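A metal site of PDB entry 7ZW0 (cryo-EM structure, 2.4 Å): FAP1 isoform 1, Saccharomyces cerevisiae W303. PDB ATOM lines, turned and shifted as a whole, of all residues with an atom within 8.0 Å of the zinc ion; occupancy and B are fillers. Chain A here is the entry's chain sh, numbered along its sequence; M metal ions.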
ATOM      1  N   MET A  69     -13.082 -10.220  32.350  1.00  0.00           N
ATOM      2  CA  MET A  69     -12.785  -9.893  30.955  1.00  0.00           C
ATOM      3  C   MET A  69     -12.132  -8.545  30.682  1.00  0.00           C
ATOM      4  O   MET A  69     -11.205  -8.467  29.879  1.00  0.00           O
ATOM      5  CB  MET A  69     -14.047 -10.042  30.106  1.00  0.00           C
ATOM      6  CG  MET A  69     -14.576 -11.462  30.060  1.00  0.00           C
ATOM      7  SD  MET A  69     -15.960 -11.688  28.921  1.00  0.00           S
ATOM      8  CE  MET A  69     -15.180 -11.294  27.360  1.00  0.00           C
ATOM      9  N   PHE A  82     -19.804  -9.396  38.462  1.00  0.00           N
ATOM     10  CA  PHE A  82     -21.021  -8.887  37.810  1.00  0.00           C
ATOM     11  C   PHE A  82     -21.575  -9.916  36.821  1.00  0.00           C
ATOM     12  O   PHE A  82     -20.807 -10.498  36.052  1.00  0.00           O
ATOM     13  CB  PHE A  82     -20.738  -7.594  37.077  1.00  0.00           C
ATOM     14  CG  PHE A  82     -21.926  -7.056  36.326  1.00  0.00           C
ATOM     15  CD1 PHE A  82     -22.946  -6.417  37.003  1.00  0.00           C
ATOM     16  CD2 PHE A  82     -22.012  -7.181  34.956  1.00  0.00           C
ATOM     17  CE1 PHE A  82     -24.048  -5.920  36.324  1.00  0.00           C
ATOM     18  CE2 PHE A  82     -23.105  -6.702  34.267  1.00  0.00           C
ATOM     19  CZ  PHE A  82     -24.117  -6.062  34.951  1.00  0.00           C
ATOM     20  N   ALA A  83     -22.876 -10.151  36.845  1.00  0.00           N
ATOM     21  CA  ALA A  83     -23.465 -11.163  35.976  1.00  0.00           C
ATOM     22  C   ALA A  83     -24.445 -10.577  34.984  1.00  0.00           C
ATOM     23  O   ALA A  83     -25.260  -9.722  35.333  1.00  0.00           O
ATOM     24  CB  ALA A  83     -24.118 -12.251  36.799  1.00  0.00           C
ATOM     25  N   CYS A  84     -24.386 -11.037  33.745  1.00  0.00           N
ATOM     26  CA  CYS A  84     -25.333 -10.581  32.737  1.00  0.00           C
ATOM     27  C   CYS A  84     -26.144 -11.773  32.293  1.00  0.00           C
ATOM     28  O   CYS A  84     -25.580 -12.819  32.009  1.00  0.00           O
ATOM     29  CB  CYS A  84     -24.619  -9.955  31.540  1.00  0.00           C
ATOM     30  SG  CYS A  84     -25.698  -9.580  30.146  1.00  0.00           S
ATOM     31  N   LYS A  85     -27.458 -11.636  32.228  1.00  0.00           N
ATOM     32  CA  LYS A  85     -28.294 -12.776  31.889  1.00  0.00           C
ATOM     33  C   LYS A  85     -28.012 -13.291  30.493  1.00  0.00           C
ATOM     34  O   LYS A  85     -27.990 -14.491  30.265  1.00  0.00           O
ATOM     35  CB  LYS A  85     -29.784 -12.411  32.023  1.00  0.00           C
ATOM     36  CG  LYS A  85     -30.315 -12.393  33.457  1.00  0.00           C
ATOM     37  CD  LYS A  85     -29.989 -11.093  34.184  1.00  0.00           C
ATOM     38  CE  LYS A  85     -28.933 -11.298  35.247  1.00  0.00           C
ATOM     39  NZ  LYS A  85     -28.378 -10.003  35.728  1.00  0.00           N
ATOM     40  N   ARG A  86     -27.783 -12.388  29.551  1.00  0.00           N
ATOM     41  CA  ARG A  86     -27.574 -12.806  28.174  1.00  0.00           C
ATOM     42  C   ARG A  86     -26.323 -13.679  28.005  1.00  0.00           C
ATOM     43  O   ARG A  86     -26.369 -14.697  27.311  1.00  0.00           O
ATOM     44  CB  ARG A  86     -27.519 -11.584  27.250  1.00  0.00           C
ATOM     45  CG  ARG A  86     -27.731 -11.917  25.780  1.00  0.00           C
ATOM     46  CD  ARG A  86     -29.110 -12.500  25.544  1.00  0.00           C
ATOM     47  NE  ARG A  86     -29.201 -13.203  24.268  1.00  0.00           N
ATOM     48  CZ  ARG A  86     -28.987 -14.507  24.113  1.00  0.00           C
ATOM     49  NH1 ARG A  86     -28.677 -15.255  25.159  1.00  0.00           N
ATOM     50  NH2 ARG A  86     -29.082 -15.064  22.911  1.00  0.00           N
ATOM     51  N   CYS A  87     -25.225 -13.300  28.645  1.00  0.00           N
ATOM     52  CA  CYS A  87     -23.998 -14.086  28.529  1.00  0.00           C
ATOM     53  C   CYS A  87     -23.735 -15.018  29.692  1.00  0.00           C
ATOM     54  O   CYS A  87     -22.855 -15.875  29.594  1.00  0.00           O
ATOM     55  CB  CYS A  87     -22.798 -13.160  28.391  1.00  0.00           C
ATOM     56  SG  CYS A  87     -22.396 -12.265  29.907  1.00  0.00           S
ATOM     57  N   TYR A  88     -24.495 -14.894  30.767  1.00  0.00           N
ATOM     58  CA  TYR A  88     -24.237 -15.681  31.974  1.00  0.00           C
ATOM     59  C   TYR A  88     -22.749 -15.854  32.257  1.00  0.00           C
ATOM     60  O   TYR A  88     -22.285 -16.964  32.541  1.00  0.00           O
ATOM     61  CB  TYR A  88     -24.983 -17.016  31.950  1.00  0.00           C
ATOM     62  CG  TYR A  88     -26.420 -16.866  32.381  1.00  0.00           C
ATOM     63  CD1 TYR A  88     -26.731 -16.208  33.566  1.00  0.00           C
ATOM     64  CD2 TYR A  88     -27.453 -17.382  31.624  1.00  0.00           C
ATOM     65  CE1 TYR A  88     -28.043 -16.061  33.971  1.00  0.00           C
ATOM     66  CE2 TYR A  88     -28.768 -17.241  32.017  1.00  0.00           C
ATOM     67  CZ  TYR A  88     -29.059 -16.569  33.193  1.00  0.00           C
ATOM     68  OH  TYR A  88     -30.366 -16.427  33.592  1.00  0.00           O
ATOM     69  N   ARG A  89     -21.998 -14.760  32.197  1.00  0.00           N
ATOM     70  CA  ARG A  89     -20.575 -14.801  32.454  1.00  0.00           C
ATOM     71  C   ARG A  89     -20.266 -13.757  33.520  1.00  0.00           C
ATOM     72  O   ARG A  89     -21.023 -12.797  33.682  1.00  0.00           O
ATOM     73  CB  ARG A  89     -19.817 -14.527  31.149  1.00  0.00           C
ATOM     74  CG  ARG A  89     -18.390 -14.019  31.269  1.00  0.00           C
ATOM     75  CD  ARG A  89     -17.372 -15.108  30.988  1.00  0.00           C
ATOM     76  NE  ARG A  89     -16.009 -14.649  31.236  1.00  0.00           N
ATOM     77  CZ  ARG A  89     -14.914 -15.372  30.993  1.00  0.00           C
ATOM     78  NH1 ARG A  89     -15.031 -16.586  30.477  1.00  0.00           N
ATOM     79  NH2 ARG A  89     -13.717 -14.876  31.267  1.00  0.00           N
ATOM     80  N   VAL A  90     -19.177 -13.921  34.256  1.00  0.00           N
ATOM     81  CA  VAL A  90     -18.844 -12.992  35.332  1.00  0.00           C
ATOM     82  C   VAL A  90     -17.539 -12.225  35.156  1.00  0.00           C
ATOM     83  O   VAL A  90     -16.527 -12.792  34.720  1.00  0.00           O
ATOM     84  CB  VAL A  90     -18.898 -13.700  36.693  1.00  0.00           C
ATOM     85  CG1 VAL A  90     -17.960 -13.082  37.700  1.00  0.00           C
ATOM     86  CG2 VAL A  90     -20.319 -13.699  37.209  1.00  0.00           C
ATOM     87  N   PHE A  91     -17.558 -10.925  35.437  1.00  0.00           N
ATOM     88  CA  PHE A  91     -16.353 -10.109  35.333  1.00  0.00           C
ATOM     89  C   PHE A  91     -16.228  -9.394  36.661  1.00  0.00           C
ATOM     90  O   PHE A  91     -17.153  -9.419  37.458  1.00  0.00           O
ATOM     91  CB  PHE A  91     -16.504  -9.078  34.215  1.00  0.00           C
ATOM     92  CG  PHE A  91     -17.627  -9.367  33.268  1.00  0.00           C
ATOM     93  CD1 PHE A  91     -18.915  -8.911  33.543  1.00  0.00           C
ATOM     94  CD2 PHE A  91     -17.410 -10.089  32.107  1.00  0.00           C
ATOM     95  CE1 PHE A  91     -19.957  -9.182  32.670  1.00  0.00           C
ATOM     96  CE2 PHE A  91     -18.441 -10.350  31.236  1.00  0.00           C
ATOM     97  CZ  PHE A  91     -19.724  -9.903  31.521  1.00  0.00           C
ATOM     98  N   ILE A  96     -15.984  -4.046  35.017  1.00  0.00           N
ATOM     99  CA  ILE A  96     -17.051  -3.959  34.039  1.00  0.00           C
ATOM    100  C   ILE A  96     -17.744  -2.589  34.095  1.00  0.00           C
ATOM    101  O   ILE A  96     -18.241  -2.114  33.074  1.00  0.00           O
ATOM    102  CB  ILE A  96     -18.064  -5.118  34.186  1.00  0.00           C
ATOM    103  CG1 ILE A  96     -18.830  -5.341  32.878  1.00  0.00           C
ATOM    104  CG2 ILE A  96     -19.058  -4.868  35.315  1.00  0.00           C
ATOM    105  CD1 ILE A  96     -17.944  -5.721  31.715  1.00  0.00           C
ATOM    106  N   TRP A 112     -24.555   1.036  27.833  1.00  0.00           N
ATOM    107  CA  TRP A 112     -23.428   0.172  28.176  1.00  0.00           C
ATOM    108  C   TRP A 112     -23.488  -1.175  27.443  1.00  0.00           C
ATOM    109  O   TRP A 112     -24.568  -1.673  27.168  1.00  0.00           O
ATOM    110  CB  TRP A 112     -23.365  -0.030  29.691  1.00  0.00           C
ATOM    111  CG  TRP A 112     -23.896  -1.334  30.174  1.00  0.00           C
ATOM    112  CD1 TRP A 112     -25.194  -1.655  30.422  1.00  0.00           C
ATOM    113  CD2 TRP A 112     -23.125  -2.512  30.485  1.00  0.00           C
ATOM    114  NE1 TRP A 112     -25.279  -2.950  30.866  1.00  0.00           N
ATOM    115  CE2 TRP A 112     -24.025  -3.497  30.907  1.00  0.00           C
ATOM    116  CE3 TRP A 112     -21.761  -2.814  30.438  1.00  0.00           C
ATOM    117  CZ2 TRP A 112     -23.614  -4.766  31.283  1.00  0.00           C
ATOM    118  CZ3 TRP A 112     -21.362  -4.070  30.810  1.00  0.00           C
ATOM    119  CH2 TRP A 112     -22.272  -5.041  31.229  1.00  0.00           C
ATOM    120  N   LYS A 113     -22.335  -1.774  27.136  1.00  0.00           N
ATOM    121  CA  LYS A 113     -22.339  -3.032  26.360  1.00  0.00           C
ATOM    122  C   LYS A 113     -21.675  -4.187  27.098  1.00  0.00           C
ATOM    123  O   LYS A 113     -20.638  -4.003  27.715  1.00  0.00           O
ATOM    124  CB  LYS A 113     -21.644  -2.815  25.010  1.00  0.00           C
ATOM    125  CG  LYS A 113     -21.815  -3.973  24.037  1.00  0.00           C
ATOM    126  CD  LYS A 113     -21.541  -3.527  22.614  1.00  0.00           C
ATOM    127  CE  LYS A 113     -22.071  -4.551  21.627  1.00  0.00           C
ATOM    128  NZ  LYS A 113     -21.966  -4.059  20.220  1.00  0.00           N
ATOM    129  N   CYS A 114     -22.262  -5.363  27.028  1.00  0.00           N
ATOM    130  CA  CYS A 114     -21.663  -6.523  27.655  1.00  0.00           C
ATOM    131  C   CYS A 114     -20.846  -7.284  26.634  1.00  0.00           C
ATOM    132  O   CYS A 114     -21.390  -7.753  25.641  1.00  0.00           O
ATOM    133  CB  CYS A 114     -22.733  -7.429  28.248  1.00  0.00           C
ATOM    134  SG  CYS A 114     -22.056  -8.865  29.101  1.00  0.00           S
ATOM    135  N   PRO A 115     -19.539  -7.436  26.867  1.00  0.00           N
ATOM    136  CA  PRO A 115     -18.653  -8.069  25.878  1.00  0.00           C
ATOM    137  C   PRO A 115     -18.881  -9.543  25.548  1.00  0.00           C
ATOM    138  O   PRO A 115     -18.801  -9.893  24.370  1.00  0.00           O
ATOM    139  CB  PRO A 115     -17.259  -7.930  26.505  1.00  0.00           C
ATOM    140  CG  PRO A 115     -17.400  -6.879  27.566  1.00  0.00           C
ATOM    141  CD  PRO A 115     -18.801  -7.003  28.067  1.00  0.00           C
ATOM    142  N   ASN A 116     -19.149 -10.382  26.532  1.00  0.00           N
ATOM    143  CA  ASN A 116     -19.260 -11.816  26.245  1.00  0.00           C
ATOM    144  C   ASN A 116     -20.402 -12.140  25.308  1.00  0.00           C
ATOM    145  O   ASN A 116     -20.250 -12.952  24.390  1.00  0.00           O
ATOM    146  CB  ASN A 116     -19.383 -12.621  27.539  1.00  0.00           C
ATOM    147  CG  ASN A 116     -19.021 -14.089  27.341  1.00  0.00           C
ATOM    148  OD1 ASN A 116     -17.940 -14.402  26.835  1.00  0.00           O
ATOM    149  ND2 ASN A 116     -19.906 -14.980  27.755  1.00  0.00           N
ATOM    150  N   CYS A 117     -21.548 -11.510  25.509  1.00  0.00           N
ATOM    151  CA  CYS A 117     -22.673 -11.711  24.606  1.00  0.00           C
ATOM    152  C   CYS A 117     -22.672 -10.649  23.537  1.00  0.00           C
ATOM    153  O   CYS A 117     -23.560 -10.641  22.679  1.00  0.00           O
ATOM    154  CB  CYS A 117     -23.989 -11.680  25.371  1.00  0.00           C
ATOM    155  SG  CYS A 117     -24.080 -10.361  26.589  1.00  0.00           S
ATOM    156  N   TYR A 118     -21.701  -9.742  23.586  1.00  0.00           N
ATOM    157  CA  TYR A 118     -21.645  -8.633  22.636  1.00  0.00           C
ATOM    158  C   TYR A 118     -23.026  -8.018  22.588  1.00  0.00           C
ATOM    159  O   TYR A 118     -23.558  -7.747  21.514  1.00  0.00           O
ATOM    160  CB  TYR A 118     -21.190  -9.117  21.248  1.00  0.00           C
ATOM    161  CG  TYR A 118     -20.578  -8.040  20.397  1.00  0.00           C
ATOM    162  CD1 TYR A 118     -19.443  -7.352  20.812  1.00  0.00           C
ATOM    163  CD2 TYR A 118     -21.126  -7.709  19.164  1.00  0.00           C
ATOM    164  CE1 TYR A 118     -18.886  -6.363  20.034  1.00  0.00           C
ATOM    165  CE2 TYR A 118     -20.571  -6.725  18.372  1.00  0.00           C
ATOM    166  CZ  TYR A 118     -19.441  -6.058  18.812  1.00  0.00           C
ATOM    167  OH  TYR A 118     -18.878  -5.074  18.027  1.00  0.00           O
ATOM    168  N   TYR A 119     -23.621  -7.801  23.756  1.00  0.00           N
ATOM    169  CA  TYR A 119     -24.986  -7.285  23.805  1.00  0.00           C
ATOM    170  C   TYR A 119     -25.054  -5.998  24.572  1.00  0.00           C
ATOM    171  O   TYR A 119     -24.574  -5.914  25.701  1.00  0.00           O
ATOM    172  CB  TYR A 119     -25.917  -8.363  24.382  1.00  0.00           C
ATOM    173  CG  TYR A 119     -26.955  -7.912  25.395  1.00  0.00           C
ATOM    174  CD1 TYR A 119     -26.671  -7.886  26.751  1.00  0.00           C
ATOM    175  CD2 TYR A 119     -28.238  -7.569  24.993  1.00  0.00           C
ATOM    176  CE1 TYR A 119     -27.610  -7.490  27.679  1.00  0.00           C
ATOM    177  CE2 TYR A 119     -29.185  -7.173  25.914  1.00  0.00           C
ATOM    178  CZ  TYR A 119     -28.868  -7.134  27.245  1.00  0.00           C
ATOM    179  OH  TYR A 119     -29.807  -6.738  28.173  1.00  0.00           O
ATOM    180  N   VAL A 120     -25.619  -4.966  23.959  1.00  0.00           N
ATOM    181  CA  VAL A 120     -25.769  -3.697  24.654  1.00  0.00           C
ATOM    182  C   VAL A 120     -26.940  -3.739  25.609  1.00  0.00           C
ATOM    183  O   VAL A 120     -27.955  -4.361  25.326  1.00  0.00           O
ATOM    184  CB  VAL A 120     -25.985  -2.551  23.654  1.00  0.00           C
ATOM    185  CG1 VAL A 120     -24.892  -1.498  23.812  1.00  0.00           C
ATOM    186  CG2 VAL A 120     -25.998  -3.088  22.241  1.00  0.00           C
ATOM    187  N   SER A 121     -26.817  -3.064  26.738  1.00  0.00           N
ATOM    188  CA  SER A 121     -27.918  -2.979  27.695  1.00  0.00           C
ATOM    189  C   SER A 121     -28.079  -1.522  28.059  1.00  0.00           C
ATOM    190  O   SER A 121     -27.187  -0.716  27.768  1.00  0.00           O
ATOM    191  CB  SER A 121     -27.677  -3.869  28.914  1.00  0.00           C
ATOM    192  OG  SER A 121     -28.797  -3.860  29.788  1.00  0.00           O
HETATM  193 ZN    ZN M   1     -23.509 -10.308  29.124  1.00  0.00          ZN
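N of Cys 114 sits at hydrogen-bond distance from O of Tyr 119, 2.7 Å away.
The side-chain sulfur (SG) of Cys 87 sits close to the backbone NH (N) of Arg 89.
The side-chain sulfur of Cys 84 sits close to the backbone NH of Arg 86 (3.5 Å).
Of the 22 residues printed, 4 come within 4 Å of the zinc ion.
The nearest printed residue that does not touch the zinc ion is Phe 91 (4.5 Å).
The zinc ion is bound by the side-chain sulfur of Cys 114 (2.0 Å), the side-chain sulfur of Cys 87 (2.4 Å), the side-chain sulfur of Cys 84 (2.5 Å) and the side-chain sulfur of Cys 117 (2.6 Å).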
